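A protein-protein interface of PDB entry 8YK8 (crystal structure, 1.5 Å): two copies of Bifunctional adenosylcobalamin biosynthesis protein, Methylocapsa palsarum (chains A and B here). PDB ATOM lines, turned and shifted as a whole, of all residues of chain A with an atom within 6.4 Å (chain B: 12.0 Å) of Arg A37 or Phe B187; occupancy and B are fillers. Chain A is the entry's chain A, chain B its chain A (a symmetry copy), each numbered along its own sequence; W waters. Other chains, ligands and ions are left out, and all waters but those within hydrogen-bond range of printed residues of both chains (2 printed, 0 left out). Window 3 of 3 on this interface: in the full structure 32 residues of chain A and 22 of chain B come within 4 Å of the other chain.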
ATOM      1  N   ASP A   9      -7.561  22.408 -11.787  1.00  0.00           N
ATOM      2  CA  ASP A   9      -8.295  21.811 -12.936  1.00  0.00           C
ATOM      3  C   ASP A   9      -9.664  22.469 -13.011  1.00  0.00           C
ATOM      4  O   ASP A   9     -10.385  22.445 -12.017  1.00  0.00           O
ATOM      5  CB  ASP A   9      -8.431  20.294 -12.799  1.00  0.00           C
ATOM      6  CG  ASP A   9      -7.089  19.619 -12.587  1.00  0.00           C
ATOM      7  OD1 ASP A   9      -6.321  19.524 -13.568  1.00  0.00           O
ATOM      8  OD2 ASP A   9      -6.806  19.247 -11.430  1.00  0.00           O
ATOM      9  N   PRO A  10     -10.045  23.091 -14.159  1.00  0.00           N
ATOM     10  CA  PRO A  10     -11.375  23.676 -14.318  1.00  0.00           C
ATOM     11  C   PRO A  10     -12.495  22.646 -14.534  1.00  0.00           C
ATOM     12  O   PRO A  10     -12.450  21.905 -15.510  1.00  0.00           O
ATOM     13  CB  PRO A  10     -11.306  24.577 -15.563  1.00  0.00           C
ATOM     14  CG  PRO A  10      -9.961  24.296 -16.204  1.00  0.00           C
ATOM     15  CD  PRO A  10      -9.190  23.327 -15.329  1.00  0.00           C
ATOM     16  N   ILE A  11     -13.522  22.696 -13.677  1.00  0.00           N
ATOM     17  CA  ILE A  11     -14.664  21.740 -13.721  1.00  0.00           C
ATOM     18  C   ILE A  11     -15.979  22.458 -13.438  1.00  0.00           C
ATOM     19  O   ILE A  11     -15.961  23.644 -13.029  1.00  0.00           O
ATOM     20  CB  ILE A  11     -14.415  20.595 -12.718  1.00  0.00           C
ATOM     21  CG1 ILE A  11     -14.237  21.120 -11.295  1.00  0.00           C
ATOM     22  CG2 ILE A  11     -13.221  19.754 -13.141  1.00  0.00           C
ATOM     23  CD1 ILE A  11     -14.264  20.011 -10.259  1.00  0.00           C
ATOM     24  N   LYS A  12     -17.096  21.759 -13.672  1.00  0.00           N
ATOM     25  CA  LYS A  12     -18.469  22.220 -13.401  1.00  0.00           C
ATOM     26  C   LYS A  12     -18.987  21.625 -12.092  1.00  0.00           C
ATOM     27  O   LYS A  12     -19.910  22.184 -11.541  1.00  0.00           O
ATOM     28  CB  LYS A  12     -19.442  21.789 -14.501  1.00  0.00           C
ATOM     29  CG  LYS A  12     -19.551  22.748 -15.680  1.00  0.00           C
ATOM     30  CD  LYS A  12     -18.537  22.510 -16.765  1.00  0.00           C
ATOM     31  CE  LYS A  12     -18.589  23.580 -17.839  1.00  0.00           C
ATOM     32  NZ  LYS A  12     -17.281  23.722 -18.515  1.00  0.00           N
ATOM     33  N   SER A  13     -18.496  20.455 -11.712  1.00  0.00           N
ATOM     34  CA  SER A  13     -19.183  19.665 -10.665  1.00  0.00           C
ATOM     35  C   SER A  13     -18.216  18.763  -9.921  1.00  0.00           C
ATOM     36  O   SER A  13     -17.437  18.083 -10.558  1.00  0.00           O
ATOM     37  CB  SER A  13     -20.338  18.883 -11.240  1.00  0.00           C
ATOM     38  OG  SER A  13     -19.922  18.039 -12.297  1.00  0.00           O
ATOM     39  N   LEU A  14     -18.277  18.826  -8.592  1.00  0.00           N
ATOM     40  CA  LEU A  14     -17.385  18.015  -7.731  1.00  0.00           C
ATOM     41  C   LEU A  14     -18.251  17.357  -6.684  1.00  0.00           C
ATOM     42  O   LEU A  14     -19.041  18.030  -6.028  1.00  0.00           O
ATOM     43  CB  LEU A  14     -16.313  18.903  -7.083  1.00  0.00           C
ATOM     44  CG  LEU A  14     -15.462  18.299  -5.960  1.00  0.00           C
ATOM     45  CD1 LEU A  14     -14.634  17.172  -6.476  1.00  0.00           C
ATOM     46  CD2 LEU A  14     -14.577  19.367  -5.325  1.00  0.00           C
ATOM     47  N   MET A  31     -11.957  24.971  -0.690  1.00  0.00           N
ATOM     48  CA  MET A  31     -11.833  24.990  -2.167  1.00  0.00           C
ATOM     49  C   MET A  31     -12.698  26.126  -2.684  1.00  0.00           C
ATOM     50  O   MET A  31     -12.297  26.847  -3.626  1.00  0.00           O
ATOM     51  CB  MET A  31     -12.263  23.710  -2.877  1.00  0.00           C
ATOM     52  CG  MET A  31     -11.765  23.709  -4.294  1.00  0.00           C
ATOM     53  SD  MET A  31      -9.990  23.531  -4.349  1.00  0.00           S
ATOM     54  CE  MET A  31      -9.814  21.996  -3.462  1.00  0.00           C
ATOM     55  N   ALA A  32     -13.903  26.264  -2.173  1.00  0.00           N
ATOM     56  CA  ALA A  32     -14.859  27.296  -2.647  1.00  0.00           C
ATOM     57  C   ALA A  32     -14.267  28.678  -2.321  1.00  0.00           C
ATOM     58  O   ALA A  32     -14.295  29.570  -3.223  1.00  0.00           O
ATOM     59  CB  ALA A  32     -16.209  27.105  -1.983  1.00  0.00           C
ATOM     60  N   GLU A  33     -13.725  28.864  -1.130  1.00  0.00           N
ATOM     61  CA  GLU A  33     -13.186  30.196  -0.730  1.00  0.00           C
ATOM     62  C   GLU A  33     -11.977  30.551  -1.594  1.00  0.00           C
ATOM     63  O   GLU A  33     -11.763  31.756  -1.849  1.00  0.00           O
ATOM     64  CB  GLU A  33     -12.914  30.250   0.751  1.00  0.00           C
ATOM     65  CG  GLU A  33     -14.199  30.311   1.514  1.00  0.00           C
ATOM     66  CD  GLU A  33     -14.022  30.191   3.003  1.00  0.00           C
ATOM     67  OE1 GLU A  33     -15.027  30.388   3.677  1.00  0.00           O
ATOM     68  OE2 GLU A  33     -12.905  29.891   3.480  1.00  0.00           O
ATOM     69  N   ALA A  34     -11.249  29.579  -2.068  1.00  0.00           N
ATOM     70  CA  ALA A  34     -10.039  29.809  -2.900  1.00  0.00           C
ATOM     71  C   ALA A  34     -10.444  30.082  -4.348  1.00  0.00           C
ATOM     72  O   ALA A  34      -9.555  30.437  -5.117  1.00  0.00           O
ATOM     73  CB  ALA A  34      -9.096  28.652  -2.855  1.00  0.00           C
ATOM     74  N   SER A  35     -11.696  29.897  -4.732  1.00  0.00           N
ATOM     75  CA  SER A  35     -12.105  29.816  -6.150  1.00  0.00           C
ATOM     76  C   SER A  35     -12.196  31.227  -6.747  1.00  0.00           C
ATOM     77  O   SER A  35     -12.041  31.339  -7.970  1.00  0.00           O
ATOM     78  CB  SER A  35     -13.403  29.095  -6.340  1.00  0.00           C
ATOM     79  OG  SER A  35     -14.513  29.836  -5.889  1.00  0.00           O
ATOM     80  N   GLY A  36     -12.585  32.191  -5.942  1.00  0.00           N
ATOM     81  CA  GLY A  36     -12.870  33.561  -6.412  1.00  0.00           C
ATOM     82  C   GLY A  36     -14.254  33.720  -6.994  1.00  0.00           C
ATOM     83  O   GLY A  36     -14.569  34.809  -7.496  1.00  0.00           O
ATOM     84  N   ARG A  37     -15.118  32.697  -6.920  1.00  0.00           N
ATOM     85  CA  ARG A  37     -16.522  32.814  -7.347  1.00  0.00           C
ATOM     86  C   ARG A  37     -17.369  33.377  -6.210  1.00  0.00           C
ATOM     87  O   ARG A  37     -16.961  33.379  -5.025  1.00  0.00           O
ATOM     88  CB  ARG A  37     -17.061  31.454  -7.821  1.00  0.00           C
ATOM     89  CG  ARG A  37     -16.394  30.911  -9.073  1.00  0.00           C
ATOM     90  CD  ARG A  37     -16.610  31.793 -10.302  1.00  0.00           C
ATOM     91  NE  ARG A  37     -16.041  31.248 -11.519  1.00  0.00           N
ATOM     92  CZ  ARG A  37     -16.185  31.765 -12.737  1.00  0.00           C
ATOM     93  NH1 ARG A  37     -16.814  32.924 -12.887  1.00  0.00           N
ATOM     94  NH2 ARG A  37     -15.640  31.165 -13.782  1.00  0.00           N
ATOM     95  N   SER A  38     -18.584  33.811  -6.548  1.00  0.00           N
ATOM     96  CA  SER A  38     -19.583  34.237  -5.556  1.00  0.00           C
ATOM     97  C   SER A  38     -20.059  32.967  -4.856  1.00  0.00           C
ATOM     98  O   SER A  38     -20.511  32.093  -5.599  1.00  0.00           O
ATOM     99  CB  SER A  38     -20.722  34.984  -6.193  1.00  0.00           C
ATOM    100  OG  SER A  38     -21.752  35.214  -5.234  1.00  0.00           O
ATOM    101  N   LEU A  39     -19.931  32.894  -3.538  1.00  0.00           N
ATOM    102  CA  LEU A  39     -20.182  31.637  -2.791  1.00  0.00           C
ATOM    103  C   LEU A  39     -21.617  31.594  -2.307  1.00  0.00           C
ATOM    104  O   LEU A  39     -22.084  32.573  -1.731  1.00  0.00           O
ATOM    105  CB  LEU A  39     -19.186  31.563  -1.642  1.00  0.00           C
ATOM    106  CG  LEU A  39     -17.743  31.471  -2.114  1.00  0.00           C
ATOM    107  CD1 LEU A  39     -16.833  31.051  -0.975  1.00  0.00           C
ATOM    108  CD2 LEU A  39     -17.659  30.502  -3.269  1.00  0.00           C
ATOM    109  N   PRO A  86     -23.156  31.161 -13.756  1.00  0.00           N
ATOM    110  CA  PRO A  86     -21.740  31.048 -14.106  1.00  0.00           C
ATOM    111  C   PRO A  86     -20.802  31.682 -13.058  1.00  0.00           C
ATOM    112  O   PRO A  86     -19.736  31.171 -12.825  1.00  0.00           O
ATOM    113  CB  PRO A  86     -21.607  31.836 -15.425  1.00  0.00           C
ATOM    114  CG  PRO A  86     -23.022  31.988 -15.965  1.00  0.00           C
ATOM    115  CD  PRO A  86     -23.994  31.671 -14.854  1.00  0.00           C
ATOM    116  N   GLU A  87     -21.226  32.787 -12.459  1.00  0.00           N
ATOM    117  CA  GLU A  87     -20.382  33.624 -11.566  1.00  0.00           C
ATOM    118  C   GLU A  87     -20.452  33.074 -10.132  1.00  0.00           C
ATOM    119  O   GLU A  87     -19.731  33.554  -9.260  1.00  0.00           O
ATOM    120  CB  GLU A  87     -20.783  35.104 -11.689  1.00  0.00           C
ATOM    121  CG  GLU A  87     -22.183  35.440 -11.187  1.00  0.00           C
ATOM    122  CD  GLU A  87     -23.352  35.315 -12.164  1.00  0.00           C
ATOM    123  OE1 GLU A  87     -23.141  34.992 -13.371  1.00  0.00           O
ATOM    124  OE2 GLU A  87     -24.490  35.529 -11.718  1.00  0.00           O
ATOM    125  N   ARG A  88     -21.312  32.095  -9.871  1.00  0.00           N
ATOM    126  CA  ARG A  88     -21.604  31.578  -8.515  1.00  0.00           C
ATOM    127  C   ARG A  88     -20.989  30.187  -8.397  1.00  0.00           C
ATOM    128  O   ARG A  88     -20.819  29.512  -9.444  1.00  0.00           O
ATOM    129  CB  ARG A  88     -23.099  31.452  -8.255  1.00  0.00           C
ATOM    130  CG  ARG A  88     -23.713  32.681  -7.598  1.00  0.00           C
ATOM    131  CD  ARG A  88     -25.207  32.572  -7.580  1.00  0.00           C
ATOM    132  NE  ARG A  88     -25.771  33.415  -6.563  1.00  0.00           N
ATOM    133  CZ  ARG A  88     -26.965  33.258  -6.016  1.00  0.00           C
ATOM    134  NH1 ARG A  88     -27.761  32.255  -6.378  1.00  0.00           N
ATOM    135  NH2 ARG A  88     -27.344  34.080  -5.064  1.00  0.00           N
ATOM    136  N   LEU A  89     -20.544  29.867  -7.186  1.00  0.00           N
ATOM    137  CA  LEU A  89     -20.266  28.446  -6.849  1.00  0.00           C
ATOM    138  C   LEU A  89     -21.218  28.032  -5.752  1.00  0.00           C
ATOM    139  O   LEU A  89     -21.199  28.625  -4.689  1.00  0.00           O
ATOM    140  CB  LEU A  89     -18.823  28.306  -6.383  1.00  0.00           C
ATOM    141  CG  LEU A  89     -18.379  26.920  -5.875  1.00  0.00           C
ATOM    142  CD1 LEU A  89     -18.661  25.853  -6.912  1.00  0.00           C
ATOM    143  CD2 LEU A  89     -16.901  26.966  -5.557  1.00  0.00           C
ATOM    144  N   PRO A 126     -21.264  26.245 -11.521  1.00  0.00           N
ATOM    145  CA  PRO A 126     -20.605  25.154 -10.797  1.00  0.00           C
ATOM    146  C   PRO A 126     -21.146  24.862  -9.398  1.00  0.00           C
ATOM    147  O   PRO A 126     -21.822  25.654  -8.796  1.00  0.00           O
ATOM    148  CB  PRO A 126     -19.167  25.613 -10.672  1.00  0.00           C
ATOM    149  CG  PRO A 126     -19.306  27.118 -10.644  1.00  0.00           C
ATOM    150  CD  PRO A 126     -20.406  27.432 -11.651  1.00  0.00           C
ATOM    151  N   VAL A 127     -20.919  23.602  -8.972  1.00  0.00           N
ATOM    152  CA  VAL A 127     -21.502  23.044  -7.729  1.00  0.00           C
ATOM    153  C   VAL A 127     -20.504  22.048  -7.113  1.00  0.00           C
ATOM    154  O   VAL A 127     -19.840  21.265  -7.829  1.00  0.00           O
ATOM    155  CB  VAL A 127     -22.862  22.374  -8.017  1.00  0.00           C
ATOM    156  CG1 VAL A 127     -22.724  21.226  -9.039  1.00  0.00           C
ATOM    157  CG2 VAL A 127     -23.552  21.899  -6.762  1.00  0.00           C
ATOM    158  N   ILE A 128     -20.398  22.125  -5.804  1.00  0.00           N
ATOM    159  CA  ILE A 128     -19.720  21.074  -5.001  1.00  0.00           C
ATOM    160  C   ILE A 128     -20.800  20.431  -4.154  1.00  0.00           C
ATOM    161  O   ILE A 128     -21.574  21.121  -3.430  1.00  0.00           O
ATOM    162  CB  ILE A 128     -18.591  21.628  -4.116  1.00  0.00           C
ATOM    163  CG1 ILE A 128     -17.558  22.383  -4.929  1.00  0.00           C
ATOM    164  CG2 ILE A 128     -17.967  20.479  -3.334  1.00  0.00           C
ATOM    165  CD1 ILE A 128     -16.579  23.162  -4.060  1.00  0.00           C
ATOM    166  N   PRO B 183      -5.738  17.323  -4.253  1.00  0.00           N
ATOM    167  CA  PRO B 183      -6.329  17.839  -5.465  1.00  0.00           C
ATOM    168  C   PRO B 183      -6.784  19.291  -5.310  1.00  0.00           C
ATOM    169  O   PRO B 183      -7.142  19.720  -4.208  1.00  0.00           O
ATOM    170  CB  PRO B 183      -7.528  16.915  -5.783  1.00  0.00           C
ATOM    171  CG  PRO B 183      -7.754  16.093  -4.554  1.00  0.00           C
ATOM    172  CD  PRO B 183      -6.538  16.222  -3.676  1.00  0.00           C
ATOM    173  N   VAL B 184      -6.720  20.023  -6.414  1.00  0.00           N
ATOM    174  CA  VAL B 184      -7.174  21.430  -6.525  1.00  0.00           C
ATOM    175  C   VAL B 184      -8.098  21.483  -7.732  1.00  0.00           C
ATOM    176  O   VAL B 184      -7.772  20.867  -8.773  1.00  0.00           O
ATOM    177  CB  VAL B 184      -5.978  22.403  -6.683  1.00  0.00           C
ATOM    178  CG1 VAL B 184      -6.412  23.851  -6.586  1.00  0.00           C
ATOM    179  CG2 VAL B 184      -4.912  22.139  -5.661  1.00  0.00           C
ATOM    180  N   PHE B 185      -9.187  22.215  -7.600  1.00  0.00           N
ATOM    181  CA  PHE B 185     -10.168  22.433  -8.685  1.00  0.00           C
ATOM    182  C   PHE B 185     -10.407  23.932  -8.847  1.00  0.00           C
ATOM    183  O   PHE B 185     -10.556  24.665  -7.817  1.00  0.00           O
ATOM    184  CB  PHE B 185     -11.419  21.599  -8.409  1.00  0.00           C
ATOM    185  CG  PHE B 185     -11.144  20.125  -8.268  1.00  0.00           C
ATOM    186  CD1 PHE B 185     -10.843  19.340  -9.364  1.00  0.00           C
ATOM    187  CD2 PHE B 185     -11.141  19.541  -7.017  1.00  0.00           C
ATOM    188  CE1 PHE B 185     -10.590  17.983  -9.214  1.00  0.00           C
ATOM    189  CE2 PHE B 185     -10.872  18.199  -6.866  1.00  0.00           C
ATOM    190  CZ  PHE B 185     -10.622  17.409  -7.961  1.00  0.00           C
ATOM    191  N   ARG B 186     -10.463  24.367 -10.106  1.00  0.00           N
ATOM    192  CA  ARG B 186     -10.980  25.704 -10.492  1.00  0.00           C
ATOM    193  C   ARG B 186     -12.422  25.555 -10.983  1.00  0.00           C
ATOM    194  O   ARG B 186     -12.724  24.541 -11.656  1.00  0.00           O
ATOM    195  CB  ARG B 186     -10.227  26.375 -11.645  1.00  0.00           C
ATOM    196  CG  ARG B 186     -10.675  27.826 -11.794  1.00  0.00           C
ATOM    197  CD  ARG B 186     -10.117  28.697 -12.896  1.00  0.00           C
ATOM    198  NE  ARG B 186     -10.599  28.365 -14.221  1.00  0.00           N
ATOM    199  CZ  ARG B 186      -9.875  27.890 -15.214  1.00  0.00           C
ATOM    200  NH1 ARG B 186      -8.586  27.629 -15.065  1.00  0.00           N
ATOM    201  NH2 ARG B 186     -10.459  27.663 -16.376  1.00  0.00           N
ATOM    202  N   PHE B 187     -13.271  26.536 -10.674  1.00  0.00           N
ATOM    203  CA  PHE B 187     -14.699  26.589 -11.068  1.00  0.00           C
ATOM    204  C   PHE B 187     -15.021  27.862 -11.875  1.00  0.00           C
ATOM    205  O   PHE B 187     -14.320  28.830 -11.584  1.00  0.00           O
ATOM    206  CB  PHE B 187     -15.570  26.506  -9.822  1.00  0.00           C
ATOM    207  CG  PHE B 187     -15.331  25.241  -9.038  1.00  0.00           C
ATOM    208  CD1 PHE B 187     -15.976  24.073  -9.396  1.00  0.00           C
ATOM    209  CD2 PHE B 187     -14.555  25.259  -7.895  1.00  0.00           C
ATOM    210  CE1 PHE B 187     -15.784  22.923  -8.652  1.00  0.00           C
ATOM    211  CE2 PHE B 187     -14.371  24.112  -7.147  1.00  0.00           C
ATOM    212  CZ  PHE B 187     -14.974  22.952  -7.545  1.00  0.00           C
HETATM  213  O   HOH W   1     -10.550  26.872  -5.944  1.00  0.00           O
HETATM  214  O   HOH W   2     -12.378  29.323  -9.790  1.00  0.00           O
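The backbone NH (N) of Asp A9 sits at hydrogen-bond distance from the backbone carbonyl oxygen (O) of Val B184 (3.4 Å). N of Ile A11 sits at hydrogen-bond distance from O of Arg B186 (2.9 Å). N of Phe B185 lies within hydrogen-bond range of SD of Met A31 (3.6 Å). The backbone carbonyl oxygen of Phe B187 sits at hydrogen-bond distance from the guanidinium group of Arg A37. The backbone NH (N) of Arg B186 is in hydrogen-bond range of the backbone carbonyl oxygen (O) of Asp A9, 2.7 Å away.
NH1 of Arg A37 sits at hydrogen-bond distance from O of Pro A86. OG of Ser A35 sits at hydrogen-bond distance from N of Arg A37 (3.1 Å). N of Leu A14 lies within hydrogen-bond range of O of Val A127 (3.0 Å). The backbone carbonyl oxygen of Ser A38 lies within hydrogen-bond range of the backbone NH of Leu A89, at 2.7 Å.
Among the printed residues, pairs that only touch across the chains: Pro A10 with Arg B186, Asp A9 with Phe B185, Ile A11 with Phe B187, Met A31 with Pro B183, Ile A11 with Phe B185, Ile A128 with Phe B187, Leu A89 with Phe B187, Pro A126 with Phe B187, Leu A14 with Phe B185 and Met A31 with Phe B187.
Phe B187 touches just these residues of chain A: Ile A11 (3.6 Å), Met A31 (3.9 Å), Arg A37 (3.0 Å), Leu A89 (3.7 Å), Pro A126 (3.8 Å) and Ile A128 (3.7 Å). Pro A10 touches just one residue of chain B: Arg B186. Of chain B, only Phe B185 (3.8 Å) comes within 4 Å of Leu A14. Of chain B, only Pro B183, Phe B185 and Phe B187 come within 4 Å of Met A31. No residue of chain B comes within 4 Å of Ala A32. No residue of chain B comes within 4 Å of Ser A35. No residue of chain B comes within 4 Å of Gly A36. No residue of chain B comes within 4 Å of Ser A38. No residue of chain B comes within 4 Å of Leu A39. Leu A89 touches one residue of chain B. Pro A126 touches just one residue of chain B: Phe B187 (3.8 Å). Of the printed residues of chain A, Arg B186 touches Asp A9, Pro A10 and Ile A11. Printed residues of chain A within 4 Å of Pro B183: Met A31. Of the printed residues of chain B, Asp A9 touches Val B184 (3.3 Å), Phe B185 (3.3 Å) and Arg B186 (2.7 Å). Of the printed residues of chain A, Phe B185 touches Asp A9 (3.3 Å), Ile A11 (3.6 Å), Leu A14 (3.8 Å) and Met A31 (3.6 Å). The nearest residue of chain B that does not touch Arg A37 is Arg B186 (5.8 Å).
Printed residues of chain B that touch a printed residue of chain A: Pro B183, Val B184, Phe B185, Arg B186 and Phe B187. Among the printed residues, 15 pairs touch across the chains. Among the printed residues, no Asp or Glu carboxylate lies within 4 Å of a Lys or Arg side-chain nitrogen of the other chain.
No position is printed for both chains.
Water W2 bridges O of Phe B187 (2.7 Å) and O of Ser A35 (2.7 Å). Water W1 lies within hydrogen-bond range of O of Phe B185 (2.9 Å), O of Met A31 (2.9 Å) and N of Ser A35 (3.5 Å).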
